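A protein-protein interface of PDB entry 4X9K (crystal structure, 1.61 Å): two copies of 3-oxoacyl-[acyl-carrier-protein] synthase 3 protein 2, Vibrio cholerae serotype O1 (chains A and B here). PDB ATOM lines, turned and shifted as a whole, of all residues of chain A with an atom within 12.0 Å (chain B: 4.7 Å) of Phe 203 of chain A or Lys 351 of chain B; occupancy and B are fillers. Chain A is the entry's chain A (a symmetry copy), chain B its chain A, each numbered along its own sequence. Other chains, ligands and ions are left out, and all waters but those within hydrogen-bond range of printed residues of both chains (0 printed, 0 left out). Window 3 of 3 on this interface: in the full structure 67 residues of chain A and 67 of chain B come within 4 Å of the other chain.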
ATOM      1  N   LYS A 195      10.856 -19.462  -0.316  1.00  0.00           N
ATOM      2  CA  LYS A 195      10.056 -18.548   0.518  1.00  0.00           C
ATOM      3  C   LYS A 195      10.831 -17.832   1.632  1.00  0.00           C
ATOM      4  O   LYS A 195      10.278 -17.487   2.689  1.00  0.00           O
ATOM      5  CB  LYS A 195       8.836 -19.291   1.073  1.00  0.00           C
ATOM      6  CG  LYS A 195       7.908 -19.816  -0.008  1.00  0.00           C
ATOM      7  CD  LYS A 195       7.287 -18.705  -0.840  1.00  0.00           C
ATOM      8  CE  LYS A 195       6.215 -19.260  -1.766  1.00  0.00           C
ATOM      9  NZ  LYS A 195       5.686 -18.220  -2.688  1.00  0.00           N
ATOM     10  N   PHE A 196      12.109 -17.544   1.375  1.00  0.00           N
ATOM     11  CA  PHE A 196      12.762 -16.457   2.070  1.00  0.00           C
ATOM     12  C   PHE A 196      13.190 -15.441   1.021  1.00  0.00           C
ATOM     13  O   PHE A 196      14.025 -15.738   0.157  1.00  0.00           O
ATOM     14  CB  PHE A 196      13.983 -16.847   2.901  1.00  0.00           C
ATOM     15  CG  PHE A 196      14.582 -15.654   3.589  1.00  0.00           C
ATOM     16  CD1 PHE A 196      13.934 -15.074   4.675  1.00  0.00           C
ATOM     17  CD2 PHE A 196      15.698 -15.003   3.062  1.00  0.00           C
ATOM     18  CE1 PHE A 196      14.431 -13.942   5.281  1.00  0.00           C
ATOM     19  CE2 PHE A 196      16.180 -13.859   3.655  1.00  0.00           C
ATOM     20  CZ  PHE A 196      15.565 -13.322   4.763  1.00  0.00           C
ATOM     21  N   GLY A 197      12.627 -14.245   1.125  1.00  0.00           N
ATOM     22  CA  GLY A 197      12.822 -13.178   0.148  1.00  0.00           C
ATOM     23  C   GLY A 197      11.498 -12.471  -0.032  1.00  0.00           C
ATOM     24  O   GLY A 197      10.588 -12.682   0.764  1.00  0.00           O
ATOM     25  N   THR A 198      11.363 -11.641  -1.063  1.00  0.00           N
ATOM     26  CA  THR A 198      10.108 -10.898  -1.236  1.00  0.00           C
ATOM     27  C   THR A 198       8.966 -11.772  -1.768  1.00  0.00           C
ATOM     28  O   THR A 198       7.844 -11.282  -1.889  1.00  0.00           O
ATOM     29  CB  THR A 198      10.280  -9.632  -2.122  1.00  0.00           C
ATOM     30  OG1 THR A 198      10.590 -10.016  -3.469  1.00  0.00           O
ATOM     31  CG2 THR A 198      11.386  -8.738  -1.567  1.00  0.00           C
ATOM     32  N   ALA A 199       9.232 -13.036  -2.078  1.00  0.00           N
ATOM     33  CA  ALA A 199       8.184 -14.011  -2.401  1.00  0.00           C
ATOM     34  C   ALA A 199       7.415 -14.433  -1.140  1.00  0.00           C
ATOM     35  O   ALA A 199       6.323 -14.993  -1.253  1.00  0.00           O
ATOM     36  CB  ALA A 199       8.761 -15.246  -3.086  1.00  0.00           C
ATOM     37  N   MET A 200       7.976 -14.195   0.042  1.00  0.00           N
ATOM     38  CA  MET A 200       7.370 -14.682   1.284  1.00  0.00           C
ATOM     39  C   MET A 200       6.258 -13.735   1.692  1.00  0.00           C
ATOM     40  O   MET A 200       6.208 -12.587   1.243  1.00  0.00           O
ATOM     41  CB  MET A 200       8.409 -14.808   2.406  1.00  0.00           C
ATOM     42  CG  MET A 200       8.778 -13.516   3.112  1.00  0.00           C
ATOM     43  SD  MET A 200      10.354 -13.581   3.996  1.00  0.00           S
ATOM     44  CE  MET A 200      10.030 -14.852   5.228  1.00  0.00           C
ATOM     45  N   ASP A 201       5.362 -14.240   2.535  1.00  0.00           N
ATOM     46  CA  ASP A 201       4.293 -13.432   3.094  1.00  0.00           C
ATOM     47  C   ASP A 201       4.820 -12.826   4.387  1.00  0.00           C
ATOM     48  O   ASP A 201       5.025 -13.519   5.385  1.00  0.00           O
ATOM     49  CB  ASP A 201       3.058 -14.297   3.336  1.00  0.00           C
ATOM     50  CG  ASP A 201       1.860 -13.502   3.844  1.00  0.00           C
ATOM     51  OD1 ASP A 201       2.013 -12.370   4.322  1.00  0.00           O
ATOM     52  OD2 ASP A 201       0.752 -14.067   3.804  1.00  0.00           O
ATOM     53  N   ARG A 202       5.036 -11.520   4.347  1.00  0.00           N
ATOM     54  CA  ARG A 202       5.612 -10.760   5.442  1.00  0.00           C
ATOM     55  C   ARG A 202       4.797 -10.859   6.736  1.00  0.00           C
ATOM     56  O   ARG A 202       5.337 -10.723   7.832  1.00  0.00           O
ATOM     57  CB  ARG A 202       5.700  -9.293   5.006  1.00  0.00           C
ATOM     58  CG  ARG A 202       6.299  -8.333   5.992  1.00  0.00           C
ATOM     59  CD  ARG A 202       6.386  -6.957   5.358  1.00  0.00           C
ATOM     60  NE  ARG A 202       6.543  -5.902   6.345  1.00  0.00           N
ATOM     61  CZ  ARG A 202       6.393  -4.600   6.099  1.00  0.00           C
ATOM     62  NH1 ARG A 202       6.127  -4.171   4.873  1.00  0.00           N
ATOM     63  NH2 ARG A 202       6.521  -3.713   7.087  1.00  0.00           N
ATOM     64  N   PHE A 203       3.499 -11.074   6.574  1.00  0.00           N
ATOM     65  CA  PHE A 203       2.564 -11.073   7.705  1.00  0.00           C
ATOM     66  C   PHE A 203       1.874 -12.419   7.928  1.00  0.00           C
ATOM     67  O   PHE A 203       0.759 -12.477   8.455  1.00  0.00           O
ATOM     68  CB  PHE A 203       1.572  -9.919   7.516  1.00  0.00           C
ATOM     69  CG  PHE A 203       2.235  -8.566   7.572  1.00  0.00           C
ATOM     70  CD1 PHE A 203       2.834  -8.129   8.746  1.00  0.00           C
ATOM     71  CD2 PHE A 203       2.323  -7.763   6.442  1.00  0.00           C
ATOM     72  CE1 PHE A 203       3.472  -6.906   8.805  1.00  0.00           C
ATOM     73  CE2 PHE A 203       2.956  -6.531   6.501  1.00  0.00           C
ATOM     74  CZ  PHE A 203       3.532  -6.102   7.687  1.00  0.00           C
ATOM     75  N   ASP A 204       2.541 -13.505   7.545  1.00  0.00           N
ATOM     76  CA  ASP A 204       2.117 -14.846   7.901  1.00  0.00           C
ATOM     77  C   ASP A 204       2.946 -15.285   9.083  1.00  0.00           C
ATOM     78  O   ASP A 204       4.183 -15.289   9.023  1.00  0.00           O
ATOM     79  CB  ASP A 204       2.295 -15.794   6.722  1.00  0.00           C
ATOM     80  CG  ASP A 204       1.822 -17.207   7.012  1.00  0.00           C
ATOM     81  OD1 ASP A 204       1.683 -17.583   8.194  1.00  0.00           O
ATOM     82  OD2 ASP A 204       1.599 -17.949   6.031  1.00  0.00           O
ATOM     83  N   ALA A 205       2.267 -15.673  10.166  1.00  0.00           N
ATOM     84  CA  ALA A 205       2.944 -16.003  11.418  1.00  0.00           C
ATOM     85  C   ALA A 205       3.782 -17.287  11.303  1.00  0.00           C
ATOM     86  O   ALA A 205       4.688 -17.516  12.113  1.00  0.00           O
ATOM     87  CB  ALA A 205       1.919 -16.138  12.551  1.00  0.00           C
ATOM     88  N   ASP A 206       3.473 -18.117  10.312  1.00  0.00           N
ATOM     89  CA  ASP A 206       4.226 -19.339  10.051  1.00  0.00           C
ATOM     90  C   ASP A 206       5.309 -19.138   8.978  1.00  0.00           C
ATOM     91  O   ASP A 206       5.867 -20.109   8.466  1.00  0.00           O
ATOM     92  CB  ASP A 206       3.284 -20.460   9.599  1.00  0.00           C
ATOM     93  CG  ASP A 206       2.362 -20.950  10.713  1.00  0.00           C
ATOM     94  OD1 ASP A 206       2.634 -20.694  11.894  1.00  0.00           O
ATOM     95  OD2 ASP A 206       1.366 -21.614  10.381  1.00  0.00           O
ATOM     96  N   ASN A 207       5.620 -17.886   8.635  1.00  0.00           N
ATOM     97  CA  ASN A 207       6.534 -17.662   7.505  1.00  0.00           C
ATOM     98  C   ASN A 207       7.983 -18.068   7.748  1.00  0.00           C
ATOM     99  O   ASN A 207       8.758 -18.135   6.798  1.00  0.00           O
ATOM    100  CB  ASN A 207       6.433 -16.221   6.966  1.00  0.00           C
ATOM    101  CG  ASN A 207       7.023 -15.179   7.884  1.00  0.00           C
ATOM    102  OD1 ASN A 207       7.563 -15.467   8.946  1.00  0.00           O
ATOM    103  ND2 ASN A 207       6.931 -13.928   7.457  1.00  0.00           N
ATOM    104  N   GLY A 208       8.348 -18.335   9.003  1.00  0.00           N
ATOM    105  CA  GLY A 208       9.694 -18.817   9.321  1.00  0.00           C
ATOM    106  C   GLY A 208       9.937 -20.281   8.983  1.00  0.00           C
ATOM    107  O   GLY A 208      11.097 -20.721   8.914  1.00  0.00           O
ATOM    108  N   TYR A 209       8.864 -21.044   8.772  1.00  0.00           N
ATOM    109  CA  TYR A 209       8.952 -22.490   8.578  1.00  0.00           C
ATOM    110  C   TYR A 209       8.964 -22.827   7.105  1.00  0.00           C
ATOM    111  O   TYR A 209       8.082 -23.515   6.593  1.00  0.00           O
ATOM    112  CB  TYR A 209       7.792 -23.198   9.316  1.00  0.00           C
ATOM    113  CG  TYR A 209       7.783 -22.818  10.768  1.00  0.00           C
ATOM    114  CD1 TYR A 209       8.737 -23.335  11.642  1.00  0.00           C
ATOM    115  CD2 TYR A 209       6.858 -21.909  11.272  1.00  0.00           C
ATOM    116  CE1 TYR A 209       8.762 -22.962  12.976  1.00  0.00           C
ATOM    117  CE2 TYR A 209       6.883 -21.526  12.604  1.00  0.00           C
ATOM    118  CZ  TYR A 209       7.827 -22.059  13.453  1.00  0.00           C
ATOM    119  OH  TYR A 209       7.853 -21.672  14.770  1.00  0.00           O
ATOM    120  N   TRP A 210       9.989 -22.326   6.417  1.00  0.00           N
ATOM    121  CA  TRP A 210      10.115 -22.527   4.980  1.00  0.00           C
ATOM    122  C   TRP A 210      10.789 -23.851   4.631  1.00  0.00           C
ATOM    123  O   TRP A 210      11.528 -24.428   5.434  1.00  0.00           O
ATOM    124  CB  TRP A 210      10.890 -21.371   4.319  1.00  0.00           C
ATOM    125  CG  TRP A 210      12.229 -21.042   4.936  1.00  0.00           C
ATOM    126  CD1 TRP A 210      13.365 -21.827   4.954  1.00  0.00           C
ATOM    127  CD2 TRP A 210      12.564 -19.838   5.611  1.00  0.00           C
ATOM    128  NE1 TRP A 210      14.371 -21.169   5.611  1.00  0.00           N
ATOM    129  CE2 TRP A 210      13.914 -19.942   6.013  1.00  0.00           C
ATOM    130  CE3 TRP A 210      11.852 -18.664   5.916  1.00  0.00           C
ATOM    131  CZ2 TRP A 210      14.562 -18.930   6.717  1.00  0.00           C
ATOM    132  CZ3 TRP A 210      12.491 -17.667   6.612  1.00  0.00           C
ATOM    133  CH2 TRP A 210      13.836 -17.795   7.003  1.00  0.00           C
ATOM    134  N   GLY B 208       7.808  -8.875  11.078  1.00  0.00           N
ATOM    135  CA  GLY B 208       7.342  -8.152   9.892  1.00  0.00           C
ATOM    136  C   GLY B 208       7.271  -6.641  10.061  1.00  0.00           C
ATOM    137  O   GLY B 208       7.193  -5.905   9.063  1.00  0.00           O
ATOM    138  N   TYR B 209       7.296  -6.165  11.306  1.00  0.00           N
ATOM    139  CA  TYR B 209       7.094  -4.750  11.612  1.00  0.00           C
ATOM    140  C   TYR B 209       8.423  -4.047  11.763  1.00  0.00           C
ATOM    141  O   TYR B 209       8.753  -3.510  12.819  1.00  0.00           O
ATOM    142  CB  TYR B 209       6.220  -4.598  12.879  1.00  0.00           C
ATOM    143  CG  TYR B 209       4.923  -5.335  12.714  1.00  0.00           C
ATOM    144  CD1 TYR B 209       3.922  -4.831  11.888  1.00  0.00           C
ATOM    145  CD2 TYR B 209       4.702  -6.557  13.341  1.00  0.00           C
ATOM    146  CE1 TYR B 209       2.735  -5.521  11.699  1.00  0.00           C
ATOM    147  CE2 TYR B 209       3.520  -7.257  13.150  1.00  0.00           C
ATOM    148  CZ  TYR B 209       2.539  -6.734  12.339  1.00  0.00           C
ATOM    149  OH  TYR B 209       1.372  -7.432  12.146  1.00  0.00           O
ATOM    150  N   LEU B 349      -2.619  -4.291  -1.390  1.00  0.00           N
ATOM    151  CA  LEU B 349      -1.929  -3.860  -0.175  1.00  0.00           C
ATOM    152  C   LEU B 349      -2.711  -4.103   1.133  1.00  0.00           C
ATOM    153  O   LEU B 349      -2.198  -3.837   2.212  1.00  0.00           O
ATOM    154  CB  LEU B 349      -1.590  -2.371  -0.262  1.00  0.00           C
ATOM    155  CG  LEU B 349      -0.628  -1.917  -1.357  1.00  0.00           C
ATOM    156  CD1 LEU B 349      -0.454  -0.416  -1.250  1.00  0.00           C
ATOM    157  CD2 LEU B 349       0.714  -2.624  -1.218  1.00  0.00           C
ATOM    158  N   SER B 350      -3.936  -4.598   1.024  1.00  0.00           N
ATOM    159  CA  SER B 350      -4.876  -4.609   2.157  1.00  0.00           C
ATOM    160  C   SER B 350      -4.326  -5.336   3.381  1.00  0.00           C
ATOM    161  O   SER B 350      -4.291  -4.763   4.474  1.00  0.00           O
ATOM    162  CB  SER B 350      -6.215  -5.208   1.720  1.00  0.00           C
ATOM    163  OG  SER B 350      -7.164  -5.138   2.778  1.00  0.00           O
ATOM    164  N   LYS B 351      -3.877  -6.581   3.198  1.00  0.00           N
ATOM    165  CA  LYS B 351      -3.307  -7.360   4.302  1.00  0.00           C
ATOM    166  C   LYS B 351      -2.181  -6.588   5.019  1.00  0.00           C
ATOM    167  O   LYS B 351      -2.162  -6.479   6.248  1.00  0.00           O
ATOM    168  CB  LYS B 351      -2.801  -8.727   3.794  1.00  0.00           C
ATOM    169  CG  LYS B 351      -2.320  -9.650   4.900  1.00  0.00           C
ATOM    170  CD  LYS B 351      -1.969 -11.050   4.421  1.00  0.00           C
ATOM    171  CE  LYS B 351      -1.728 -11.959   5.615  1.00  0.00           C
ATOM    172  NZ  LYS B 351      -1.439 -13.369   5.240  1.00  0.00           N
ATOM    173  N   ALA B 352      -1.230  -6.039   4.254  1.00  0.00           N
ATOM    174  CA  ALA B 352      -0.100  -5.332   4.857  1.00  0.00           C
ATOM    175  C   ALA B 352      -0.510  -4.049   5.593  1.00  0.00           C
ATOM    176  O   ALA B 352      -0.033  -3.768   6.695  1.00  0.00           O
ATOM    177  CB  ALA B 352       0.960  -5.019   3.796  1.00  0.00           C
ATOM    178  N   ILE B 353      -1.379  -3.260   4.980  1.00  0.00           N
ATOM    179  CA  ILE B 353      -1.875  -2.045   5.626  1.00  0.00           C
ATOM    180  C   ILE B 353      -2.582  -2.404   6.939  1.00  0.00           C
ATOM    181  O   ILE B 353      -2.289  -1.818   7.982  1.00  0.00           O
ATOM    182  CB  ILE B 353      -2.852  -1.265   4.722  1.00  0.00           C
ATOM    183  CG1 ILE B 353      -2.132  -0.712   3.483  1.00  0.00           C
ATOM    184  CG2 ILE B 353      -3.499  -0.116   5.482  1.00  0.00           C
ATOM    185  CD1 ILE B 353      -3.087  -0.385   2.352  1.00  0.00           C
ATOM    186  N   GLU B 354      -3.468  -3.392   6.871  1.00  0.00           N
ATOM    187  CA  GLU B 354      -4.251  -3.811   8.047  1.00  0.00           C
ATOM    188  C   GLU B 354      -3.343  -4.292   9.174  1.00  0.00           C
ATOM    189  O   GLU B 354      -3.534  -3.913  10.330  1.00  0.00           O
ATOM    190  CB  GLU B 354      -5.271  -4.884   7.654  1.00  0.00           C
ATOM    191  CG  GLU B 354      -6.375  -4.323   6.765  1.00  0.00           C
ATOM    192  CD  GLU B 354      -7.324  -5.377   6.223  1.00  0.00           C
ATOM    193  OE1 GLU B 354      -6.905  -6.549   6.013  1.00  0.00           O
ATOM    194  OE2 GLU B 354      -8.507  -5.026   6.003  1.00  0.00           O
ATOM    195  N   HIS B 355      -2.329  -5.094   8.848  1.00  0.00           N
ATOM    196  CA  HIS B 355      -1.402  -5.548   9.882  1.00  0.00           C
ATOM    197  C   HIS B 355      -0.579  -4.395  10.469  1.00  0.00           C
ATOM    198  O   HIS B 355      -0.384  -4.335  11.677  1.00  0.00           O
ATOM    199  CB  HIS B 355      -0.474  -6.640   9.346  1.00  0.00           C
ATOM    200  CG  HIS B 355      -1.097  -8.000   9.324  1.00  0.00           C
ATOM    201  ND1 HIS B 355      -1.936  -8.416   8.316  1.00  0.00           N
ATOM    202  CD2 HIS B 355      -1.002  -9.037  10.186  1.00  0.00           C
ATOM    203  CE1 HIS B 355      -2.336  -9.652   8.556  1.00  0.00           C
ATOM    204  NE2 HIS B 355      -1.776 -10.055   9.680  1.00  0.00           N
ATOM    205  N   CYS B 356      -0.073  -3.495   9.616  1.00  0.00           N
ATOM    206  CA  CYS B 356       0.737  -2.371  10.087  1.00  0.00           C
ATOM    207  C   CYS B 356      -0.081  -1.469  11.042  1.00  0.00           C
ATOM    208  O   CYS B 356       0.426  -0.999  12.062  1.00  0.00           O
ATOM    209  CB  CYS B 356       1.292  -1.556   8.910  1.00  0.00           C
ATOM    210  SG  CYS B 356       2.635  -2.387   8.007  1.00  0.00           S
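Among the printed residues, merely in contact across the chains: Phe 203 of chain A with Gly 208 of chain B, Phe 203 of chain A with Tyr 209 of chain B, Phe 203 of chain A with Lys 351 of chain B, Phe 203 of chain A with Ala 352 of chain B, Phe 203 of chain A with His 355 of chain B and Phe 203 of chain A with Cys 356 of chain B.
2 positions are printed for both chains. Of the 8 pairs that touch across the chains among the printed residues, none has its exchanged pair printed and touching as well.
Printed residues of chain B that touch a printed residue of chain A: Gly 208, Tyr 209, Lys 351, Ala 352, His 355 and Cys 356. Among the printed residues, 8 pairs touch across the chains. Among the printed residues, Asp or Glu carboxylates within 4 Å of a Lys or Arg side-chain nitrogen of the other chain: Asp 201 of chain A with Lys 351 of chain B (2.7 Å).
A ring nitrogen (ND1) of His 355 of chain B is in hydrogen-bond range of the backbone carbonyl oxygen of Lys 351 of chain B (2.8 Å). The backbone carbonyl oxygen (O) of Ala 352 of chain B sits at hydrogen-bond distance from the side-chain sulfur (SG) of Cys 356 of chain B (3.3 Å). N of Phe 203 of chain A lies within hydrogen-bond range of OD1 of Asp 201 of chain A (3.0 Å). The backbone NH (N) of Asp 204 of chain A lies within hydrogen-bond range of the side-chain carboxylate (OD1) of Asp 201 of chain A (3.5 Å). O of Asp 201 of chain A lies within hydrogen-bond range of ND2 of Asn 207 of chain A (2.8 Å).
The backbone carbonyl oxygen of Gly 208 of chain B lies within hydrogen-bond range of the guanidinium group of Arg 202 of chain A (2.8 Å). The side-chain amino group (NZ) of Lys 351 of chain B is in salt-bridge range of the side-chain carboxylate (OD2) of Asp 201 of chain A (2.7 Å).
Of chain B, only Gly 208 (3.9 Å), Tyr 209 (3.3 Å), Lys 351 (3.8 Å), Ala 352 (3.7 Å), His 355 (3.7 Å) and Cys 356 (3.8 Å) come within 4 Å of Phe 203 of chain A. Of chain A, only Asp 201 and Phe 203 come within 4 Å of Lys 351 of chain B. Gly 208 of chain B touches two residues of chain A. Of the printed residues of chain A, Tyr 209 of chain B touches Phe 203 (3.3 Å). Of chain A, only Phe 203 (3.7 Å) comes within 4 Å of Ala 352 of chain B. No residue of chain A comes within 4 Å of Ile 353 of chain B. His 355 of chain B touches just one residue of chain A: Phe 203. Cys 356 of chain B touches just one residue of chain A: Phe 203. Printed residues of chain B within 4 Å of Asp 201 of chain A: Lys 351. Printed residues of chain B within 4 Å of Arg 202 of chain A: Gly 208. The nearest printed residue of chain B that does not touch Phe 203 of chain A is Ile 353 of chain B (5.6 Å). The nearest printed residue of chain B that does not touch Asp 201 of chain A is His 355 of chain B (6.7 Å).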
